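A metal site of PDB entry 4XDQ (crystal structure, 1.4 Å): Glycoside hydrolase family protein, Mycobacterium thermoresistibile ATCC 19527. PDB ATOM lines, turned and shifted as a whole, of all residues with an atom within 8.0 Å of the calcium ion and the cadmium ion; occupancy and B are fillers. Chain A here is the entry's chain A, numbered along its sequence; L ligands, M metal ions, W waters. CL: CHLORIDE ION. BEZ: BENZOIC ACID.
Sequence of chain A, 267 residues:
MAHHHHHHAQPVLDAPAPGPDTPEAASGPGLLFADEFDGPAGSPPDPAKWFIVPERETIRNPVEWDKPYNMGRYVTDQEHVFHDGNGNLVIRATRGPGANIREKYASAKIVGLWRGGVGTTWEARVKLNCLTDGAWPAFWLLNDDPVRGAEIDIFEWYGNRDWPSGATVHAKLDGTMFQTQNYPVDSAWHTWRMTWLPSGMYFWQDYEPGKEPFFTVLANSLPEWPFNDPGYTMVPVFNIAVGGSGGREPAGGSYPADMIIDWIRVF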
ATOM      1  N   ASP A  35      11.265  14.846  -4.762  1.00  0.00           N
ATOM      2  CA  ASP A  35      11.801  16.130  -4.337  1.00  0.00           C
ATOM      3  C   ASP A  35      13.287  16.075  -4.646  1.00  0.00           C
ATOM      4  O   ASP A  35      14.005  15.207  -4.143  1.00  0.00           O
ATOM      5  CB  ASP A  35      11.553  16.425  -2.861  1.00  0.00           C
ATOM      6  CG  ASP A  35      11.733  17.889  -2.512  1.00  0.00           C
ATOM      7  OD1 ASP A  35      12.498  18.585  -3.218  1.00  0.00           O
ATOM      8  OD2 ASP A  35      11.097  18.352  -1.552  1.00  0.00           O
ATOM      9  N   GLU A  36      13.722  16.993  -5.507  1.00  0.00           N
ATOM     10  CA  GLU A  36      15.123  17.097  -5.894  1.00  0.00           C
ATOM     11  C   GLU A  36      15.896  18.020  -4.948  1.00  0.00           C
ATOM     12  O   GLU A  36      17.088  18.179  -5.115  1.00  0.00           O
ATOM     13  CB  GLU A  36      15.228  17.575  -7.351  1.00  0.00           C
ATOM     14  CG  GLU A  36      14.498  16.655  -8.318  1.00  0.00           C
ATOM     15  CD  GLU A  36      15.132  15.290  -8.499  1.00  0.00           C
ATOM     16  OE1 GLU A  36      16.354  15.132  -8.262  1.00  0.00           O
ATOM     17  OE2 GLU A  36      14.407  14.353  -8.904  1.00  0.00           O
ATOM     18  N   PHE A  37      15.200  18.596  -3.967  1.00  0.00           N
ATOM     19  CA  PHE A  37      15.837  19.384  -2.909  1.00  0.00           C
ATOM     20  C   PHE A  37      16.733  20.491  -3.475  1.00  0.00           C
ATOM     21  O   PHE A  37      17.813  20.767  -2.965  1.00  0.00           O
ATOM     22  CB  PHE A  37      16.562  18.475  -1.919  1.00  0.00           C
ATOM     23  CG  PHE A  37      15.629  17.553  -1.159  1.00  0.00           C
ATOM     24  CD1 PHE A  37      14.597  18.092  -0.385  1.00  0.00           C
ATOM     25  CD2 PHE A  37      15.748  16.184  -1.227  1.00  0.00           C
ATOM     26  CE1 PHE A  37      13.732  17.274   0.306  1.00  0.00           C
ATOM     27  CE2 PHE A  37      14.870  15.360  -0.534  1.00  0.00           C
ATOM     28  CZ  PHE A  37      13.869  15.915   0.229  1.00  0.00           C
ATOM     29  N   ASP A  38      16.235  21.165  -4.504  1.00  0.00           N
ATOM     30  CA  ASP A  38      17.018  22.164  -5.219  1.00  0.00           C
ATOM     31  C   ASP A  38      16.655  23.589  -4.808  1.00  0.00           C
ATOM     32  O   ASP A  38      16.892  24.535  -5.550  1.00  0.00           O
ATOM     33  CB  ASP A  38      16.863  21.975  -6.738  1.00  0.00           C
ATOM     34  CG  ASP A  38      18.129  22.315  -7.537  1.00  0.00           C
ATOM     35  OD1 ASP A  38      19.262  22.070  -7.049  1.00  0.00           O
ATOM     36  OD2 ASP A  38      17.980  22.816  -8.676  1.00  0.00           O
ATOM     37  N   GLY A  39      16.107  23.757  -3.618  1.00  0.00           N
ATOM     38  CA  GLY A  39      15.736  25.070  -3.128  1.00  0.00           C
ATOM     39  C   GLY A  39      16.890  25.946  -2.679  1.00  0.00           C
ATOM     40  O   GLY A  39      18.042  25.481  -2.562  1.00  0.00           O
ATOM     41  N   HIS A  83      17.459  23.577   3.012  1.00  0.00           N
ATOM     42  CA  HIS A  83      18.199  23.348   1.786  1.00  0.00           C
ATOM     43  C   HIS A  83      19.592  23.969   1.914  1.00  0.00           C
ATOM     44  O   HIS A  83      19.728  25.041   2.509  1.00  0.00           O
ATOM     45  CB  HIS A  83      17.515  23.978   0.580  1.00  0.00           C
ATOM     46  CG  HIS A  83      16.228  23.308   0.192  1.00  0.00           C
ATOM     47  ND1 HIS A  83      14.996  23.867   0.431  1.00  0.00           N
ATOM     48  CD2 HIS A  83      16.000  22.130  -0.417  1.00  0.00           C
ATOM     49  CE1 HIS A  83      14.054  23.057  -0.025  1.00  0.00           C
ATOM     50  NE2 HIS A  83      14.632  22.007  -0.562  1.00  0.00           N
ATOM     51  N   ASP A  84      20.602  23.341   1.342  1.00  0.00           N
ATOM     52  CA  ASP A  84      21.944  23.917   1.371  1.00  0.00           C
ATOM     53  C   ASP A  84      22.280  24.841   0.194  1.00  0.00           C
ATOM     54  O   ASP A  84      23.321  25.516   0.220  1.00  0.00           O
ATOM     55  CB  ASP A  84      23.034  22.846   1.552  1.00  0.00           C
ATOM     56  CG  ASP A  84      23.175  21.891   0.374  1.00  0.00           C
ATOM     57  OD1 ASP A  84      22.478  22.033  -0.643  1.00  0.00           O
ATOM     58  OD2 ASP A  84      24.021  20.969   0.497  1.00  0.00           O
ATOM     59  N   ASN A  86      22.988  23.827  -2.699  1.00  0.00           N
ATOM     60  CA  ASN A  86      23.866  23.048  -3.562  1.00  0.00           C
ATOM     61  C   ASN A  86      23.101  21.876  -4.147  1.00  0.00           C
ATOM     62  O   ASN A  86      23.712  20.991  -4.745  1.00  0.00           O
ATOM     63  CB  ASN A  86      25.062  22.492  -2.777  1.00  0.00           C
ATOM     64  CG  ASN A  86      25.878  23.563  -2.093  1.00  0.00           C
ATOM     65  OD1 ASN A  86      26.092  24.627  -2.667  1.00  0.00           O
ATOM     66  ND2 ASN A  86      26.333  23.296  -0.871  1.00  0.00           N
ATOM     67  N   GLY A  87      21.786  21.833  -3.948  1.00  0.00           N
ATOM     68  CA  GLY A  87      20.970  20.725  -4.427  1.00  0.00           C
ATOM     69  C   GLY A  87      20.591  19.699  -3.375  1.00  0.00           C
ATOM     70  O   GLY A  87      20.035  18.650  -3.739  1.00  0.00           O
ATOM     71  N   ASN A  88      20.861  19.960  -2.084  1.00  0.00           N
ATOM     72  CA  ASN A  88      20.521  18.998  -1.036  1.00  0.00           C
ATOM     73  C   ASN A  88      19.640  19.616   0.028  1.00  0.00           C
ATOM     74  O   ASN A  88      19.641  20.830   0.226  1.00  0.00           O
ATOM     75  CB  ASN A  88      21.784  18.487  -0.314  1.00  0.00           C
ATOM     76  CG  ASN A  88      22.871  18.091  -1.250  1.00  0.00           C
ATOM     77  OD1 ASN A  88      23.955  18.712  -1.292  1.00  0.00           O
ATOM     78  ND2 ASN A  88      22.629  17.048  -1.982  1.00  0.00           N
ATOM     79  N   LEU A  89      18.924  18.752   0.730  1.00  0.00           N
ATOM     80  CA  LEU A  89      18.369  19.072   2.024  1.00  0.00           C
ATOM     81  C   LEU A  89      19.327  18.565   3.099  1.00  0.00           C
ATOM     82  O   LEU A  89      19.921  17.501   2.948  1.00  0.00           O
ATOM     83  CB  LEU A  89      16.991  18.439   2.218  1.00  0.00           C
ATOM     84  CG  LEU A  89      16.173  19.043   3.370  1.00  0.00           C
ATOM     85  CD1 LEU A  89      15.571  20.373   2.945  1.00  0.00           C
ATOM     86  CD2 LEU A  89      15.096  18.092   3.832  1.00  0.00           C
ATOM     87  N   ARG A 125      18.948   9.460  -2.508  1.00  0.00           N
ATOM     88  CA  ARG A 125      20.397   9.583  -2.494  1.00  0.00           C
ATOM     89  C   ARG A 125      20.766  10.424  -1.271  1.00  0.00           C
ATOM     90  O   ARG A 125      20.309  11.562  -1.119  1.00  0.00           O
ATOM     91  CB  ARG A 125      20.895  10.227  -3.793  1.00  0.00           C
ATOM     92  CG  ARG A 125      22.411  10.310  -3.861  1.00  0.00           C
ATOM     93  CD  ARG A 125      22.909  10.568  -5.291  1.00  0.00           C
ATOM     94  NE  ARG A 125      24.373  10.532  -5.339  1.00  0.00           N
ATOM     95  CZ  ARG A 125      25.179  11.550  -5.075  1.00  0.00           C
ATOM     96  NH1 ARG A 125      24.714  12.767  -4.794  1.00  0.00           N
ATOM     97  NH2 ARG A 125      26.485  11.343  -5.085  1.00  0.00           N
ATOM     98  N   TRP A 189      28.417   8.750   0.148  1.00  0.00           N
ATOM     99  CA  TRP A 189      27.210   8.887  -0.648  1.00  0.00           C
ATOM    100  C   TRP A 189      26.700   7.515  -1.076  1.00  0.00           C
ATOM    101  O   TRP A 189      27.462   6.671  -1.550  1.00  0.00           O
ATOM    102  CB  TRP A 189      27.458   9.732  -1.900  1.00  0.00           C
ATOM    103  CG  TRP A 189      27.394  11.210  -1.709  1.00  0.00           C
ATOM    104  CD1 TRP A 189      28.436  12.085  -1.719  1.00  0.00           C
ATOM    105  CD2 TRP A 189      26.219  11.990  -1.484  1.00  0.00           C
ATOM    106  NE1 TRP A 189      27.984  13.353  -1.534  1.00  0.00           N
ATOM    107  CE2 TRP A 189      26.626  13.328  -1.354  1.00  0.00           C
ATOM    108  CE3 TRP A 189      24.870  11.676  -1.349  1.00  0.00           C
ATOM    109  CZ2 TRP A 189      25.725  14.372  -1.144  1.00  0.00           C
ATOM    110  CZ3 TRP A 189      23.966  12.714  -1.118  1.00  0.00           C
ATOM    111  CH2 TRP A 189      24.391  14.043  -1.007  1.00  0.00           C
ATOM    112  N   ILE A 261      20.580  15.024   1.941  1.00  0.00           N
ATOM    113  CA  ILE A 261      19.668  14.318   1.045  1.00  0.00           C
ATOM    114  C   ILE A 261      19.647  15.048  -0.293  1.00  0.00           C
ATOM    115  O   ILE A 261      19.187  16.188  -0.395  1.00  0.00           O
ATOM    116  CB  ILE A 261      18.224  14.224   1.594  1.00  0.00           C
ATOM    117  CG1 ILE A 261      18.202  13.772   3.054  1.00  0.00           C
ATOM    118  CG2 ILE A 261      17.389  13.300   0.724  1.00  0.00           C
ATOM    119  CD1 ILE A 261      16.862  13.952   3.742  1.00  0.00           C
ATOM    120  N   ASP A 262      20.153  14.383  -1.319  1.00  0.00           N
ATOM    121  CA  ASP A 262      20.173  14.959  -2.688  1.00  0.00           C
ATOM    122  C   ASP A 262      18.800  14.877  -3.356  1.00  0.00           C
ATOM    123  O   ASP A 262      18.365  15.825  -4.035  1.00  0.00           O
ATOM    124  CB  ASP A 262      21.263  14.200  -3.461  1.00  0.00           C
ATOM    125  CG  ASP A 262      21.486  14.683  -4.902  1.00  0.00           C
ATOM    126  OD1 ASP A 262      20.977  15.759  -5.310  1.00  0.00           O
ATOM    127  OD2 ASP A 262      22.212  14.030  -5.733  1.00  0.00           O
ATOM    128  N   TRP A 263      18.105  13.762  -3.175  1.00  0.00           N
ATOM    129  CA  TRP A 263      16.793  13.603  -3.778  1.00  0.00           C
ATOM    130  C   TRP A 263      16.086  12.401  -3.202  1.00  0.00           C
ATOM    131  O   TRP A 263      16.726  11.484  -2.685  1.00  0.00           O
ATOM    132  CB  TRP A 263      16.879  13.449  -5.313  1.00  0.00           C
ATOM    133  CG  TRP A 263      17.919  12.483  -5.877  1.00  0.00           C
ATOM    134  CD1 TRP A 263      19.149  12.836  -6.362  1.00  0.00           C
ATOM    135  CD2 TRP A 263      17.801  11.069  -6.076  1.00  0.00           C
ATOM    136  NE1 TRP A 263      19.790  11.748  -6.851  1.00  0.00           N
ATOM    137  CE2 TRP A 263      18.997  10.635  -6.682  1.00  0.00           C
ATOM    138  CE3 TRP A 263      16.807  10.120  -5.796  1.00  0.00           C
ATOM    139  CZ2 TRP A 263      19.223   9.312  -7.024  1.00  0.00           C
ATOM    140  CZ3 TRP A 263      17.034   8.809  -6.143  1.00  0.00           C
ATOM    141  CH2 TRP A 263      18.241   8.416  -6.759  1.00  0.00           C
ATOM    142  N   ILE A 264      14.768  12.416  -3.357  1.00  0.00           N
ATOM    143  CA  ILE A 264      13.946  11.228  -3.209  1.00  0.00           C
ATOM    144  C   ILE A 264      13.042  11.166  -4.436  1.00  0.00           C
ATOM    145  O   ILE A 264      12.506  12.212  -4.865  1.00  0.00           O
ATOM    146  CB  ILE A 264      13.112  11.214  -1.900  1.00  0.00           C
ATOM    147  CG1 ILE A 264      12.259   9.928  -1.826  1.00  0.00           C
ATOM    148  CG2 ILE A 264      12.248  12.459  -1.754  1.00  0.00           C
ATOM    149  CD1 ILE A 264      11.517   9.741  -0.509  1.00  0.00           C
ATOM    150  N   ARG A 265      12.895   9.960  -5.006  1.00  0.00           N
ATOM    151  CA  ARG A 265      12.063   9.761  -6.181  1.00  0.00           C
ATOM    152  C   ARG A 265      11.264   8.485  -5.999  1.00  0.00           C
ATOM    153  O   ARG A 265      11.773   7.502  -5.461  1.00  0.00           O
ATOM    154  CB  ARG A 265      12.932   9.619  -7.432  1.00  0.00           C
ATOM    155  CG  ARG A 265      13.717  10.872  -7.782  1.00  0.00           C
ATOM    156  CD  ARG A 265      14.793  10.593  -8.807  1.00  0.00           C
ATOM    157  NE  ARG A 265      15.650  11.769  -8.978  1.00  0.00           N
ATOM    158  CZ  ARG A 265      16.912  11.733  -9.376  1.00  0.00           C
ATOM    159  NH1 ARG A 265      17.495  10.591  -9.696  1.00  0.00           N
ATOM    160  NH2 ARG A 265      17.588  12.862  -9.457  1.00  0.00           N
HETATM  161 CL    CL L   1      23.917  16.643  -7.356  1.00  0.00          CL
HETATM  162  C   BEZ L   2      23.496  12.103  -8.402  1.00  0.00           C
HETATM  163  O1  BEZ L   2      22.255  12.184  -8.350  1.00  0.00           O
HETATM  164  O2  BEZ L   2      24.256  13.039  -8.120  1.00  0.00           O
HETATM  165  C1  BEZ L   2      24.080  10.791  -8.814  1.00  0.00           C
HETATM  166  C2  BEZ L   2      25.465  10.643  -8.923  1.00  0.00           C
HETATM  167  C3  BEZ L   2      26.006   9.414  -9.292  1.00  0.00           C
HETATM  168  C4  BEZ L   2      25.179   8.323  -9.571  1.00  0.00           C
HETATM  169  C5  BEZ L   2      23.802   8.453  -9.466  1.00  0.00           C
HETATM  170  C6  BEZ L   2      23.244   9.685  -9.093  1.00  0.00           C
HETATM  171 CA    CA M   1      19.265  17.426  -5.508  1.00  0.00          CA
HETATM  172 CD    CD M   2      22.588  14.656  -7.680  1.00  0.00          CD
HETATM  173  O   HOH W   1      19.121  19.262  -7.056  1.00  0.00           O
HETATM  174  O   HOH W   2      21.293  18.205  -6.732  1.00  0.00           O
HETATM  175  O   HOH W   3      18.555  16.282  -7.406  1.00  0.00           O
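NE1 of Trp 263 lies close to O1 of BEZ L2 (2.9 Å).
O2 of BEZ L2 lies close to NH1 of Arg 125 (3.4 Å).
The side-chain carboxylate (OD2) of Asp 262 binds the cadmium ion (2.1 Å).
The cadmium ion is bound by O2 of BEZ L2 (2.4 Å).
The cadmium ion is bound by a chlorine (CL) of CL L1, 2.4 Å away.
O1 of BEZ L2 binds the cadmium ion (2.6 Å).
The cadmium ion has four donor atoms within binding distance.
The backbone NH of Asp 262 is in hydrogen-bond range of the backbone carbonyl oxygen of Arg 125, 2.8 Å away.
OE1 of Glu 36 lies within salt-bridge range of NH2 of Arg 265.
The side-chain carboxylate (OD1) of Asp 84 lies within hydrogen-bond range of the backbone NH (N) of Gly 87 (3.4 Å).
The calcium ion is bound by O of Gly 87 (2.3 Å), water W3 (2.3 Å), O of Glu 36 (2.3 Å), O of Asp 262 (2.4 Å), OD1 of Asp 262 (2.4 Å), water W1 (2.4 Å) and water W2 (2.5 Å).
The calcium ion has seven donor atoms within binding distance.
Three residues have an atom within 4 Å of the calcium ion: Glu 36, Gly 87 and Asp 262.
The nearest printed residue that does not touch the calcium ion is Phe 37 (4.4 Å).
One residue has an atom within 4 Å of the cadmium ion: Asp 262.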
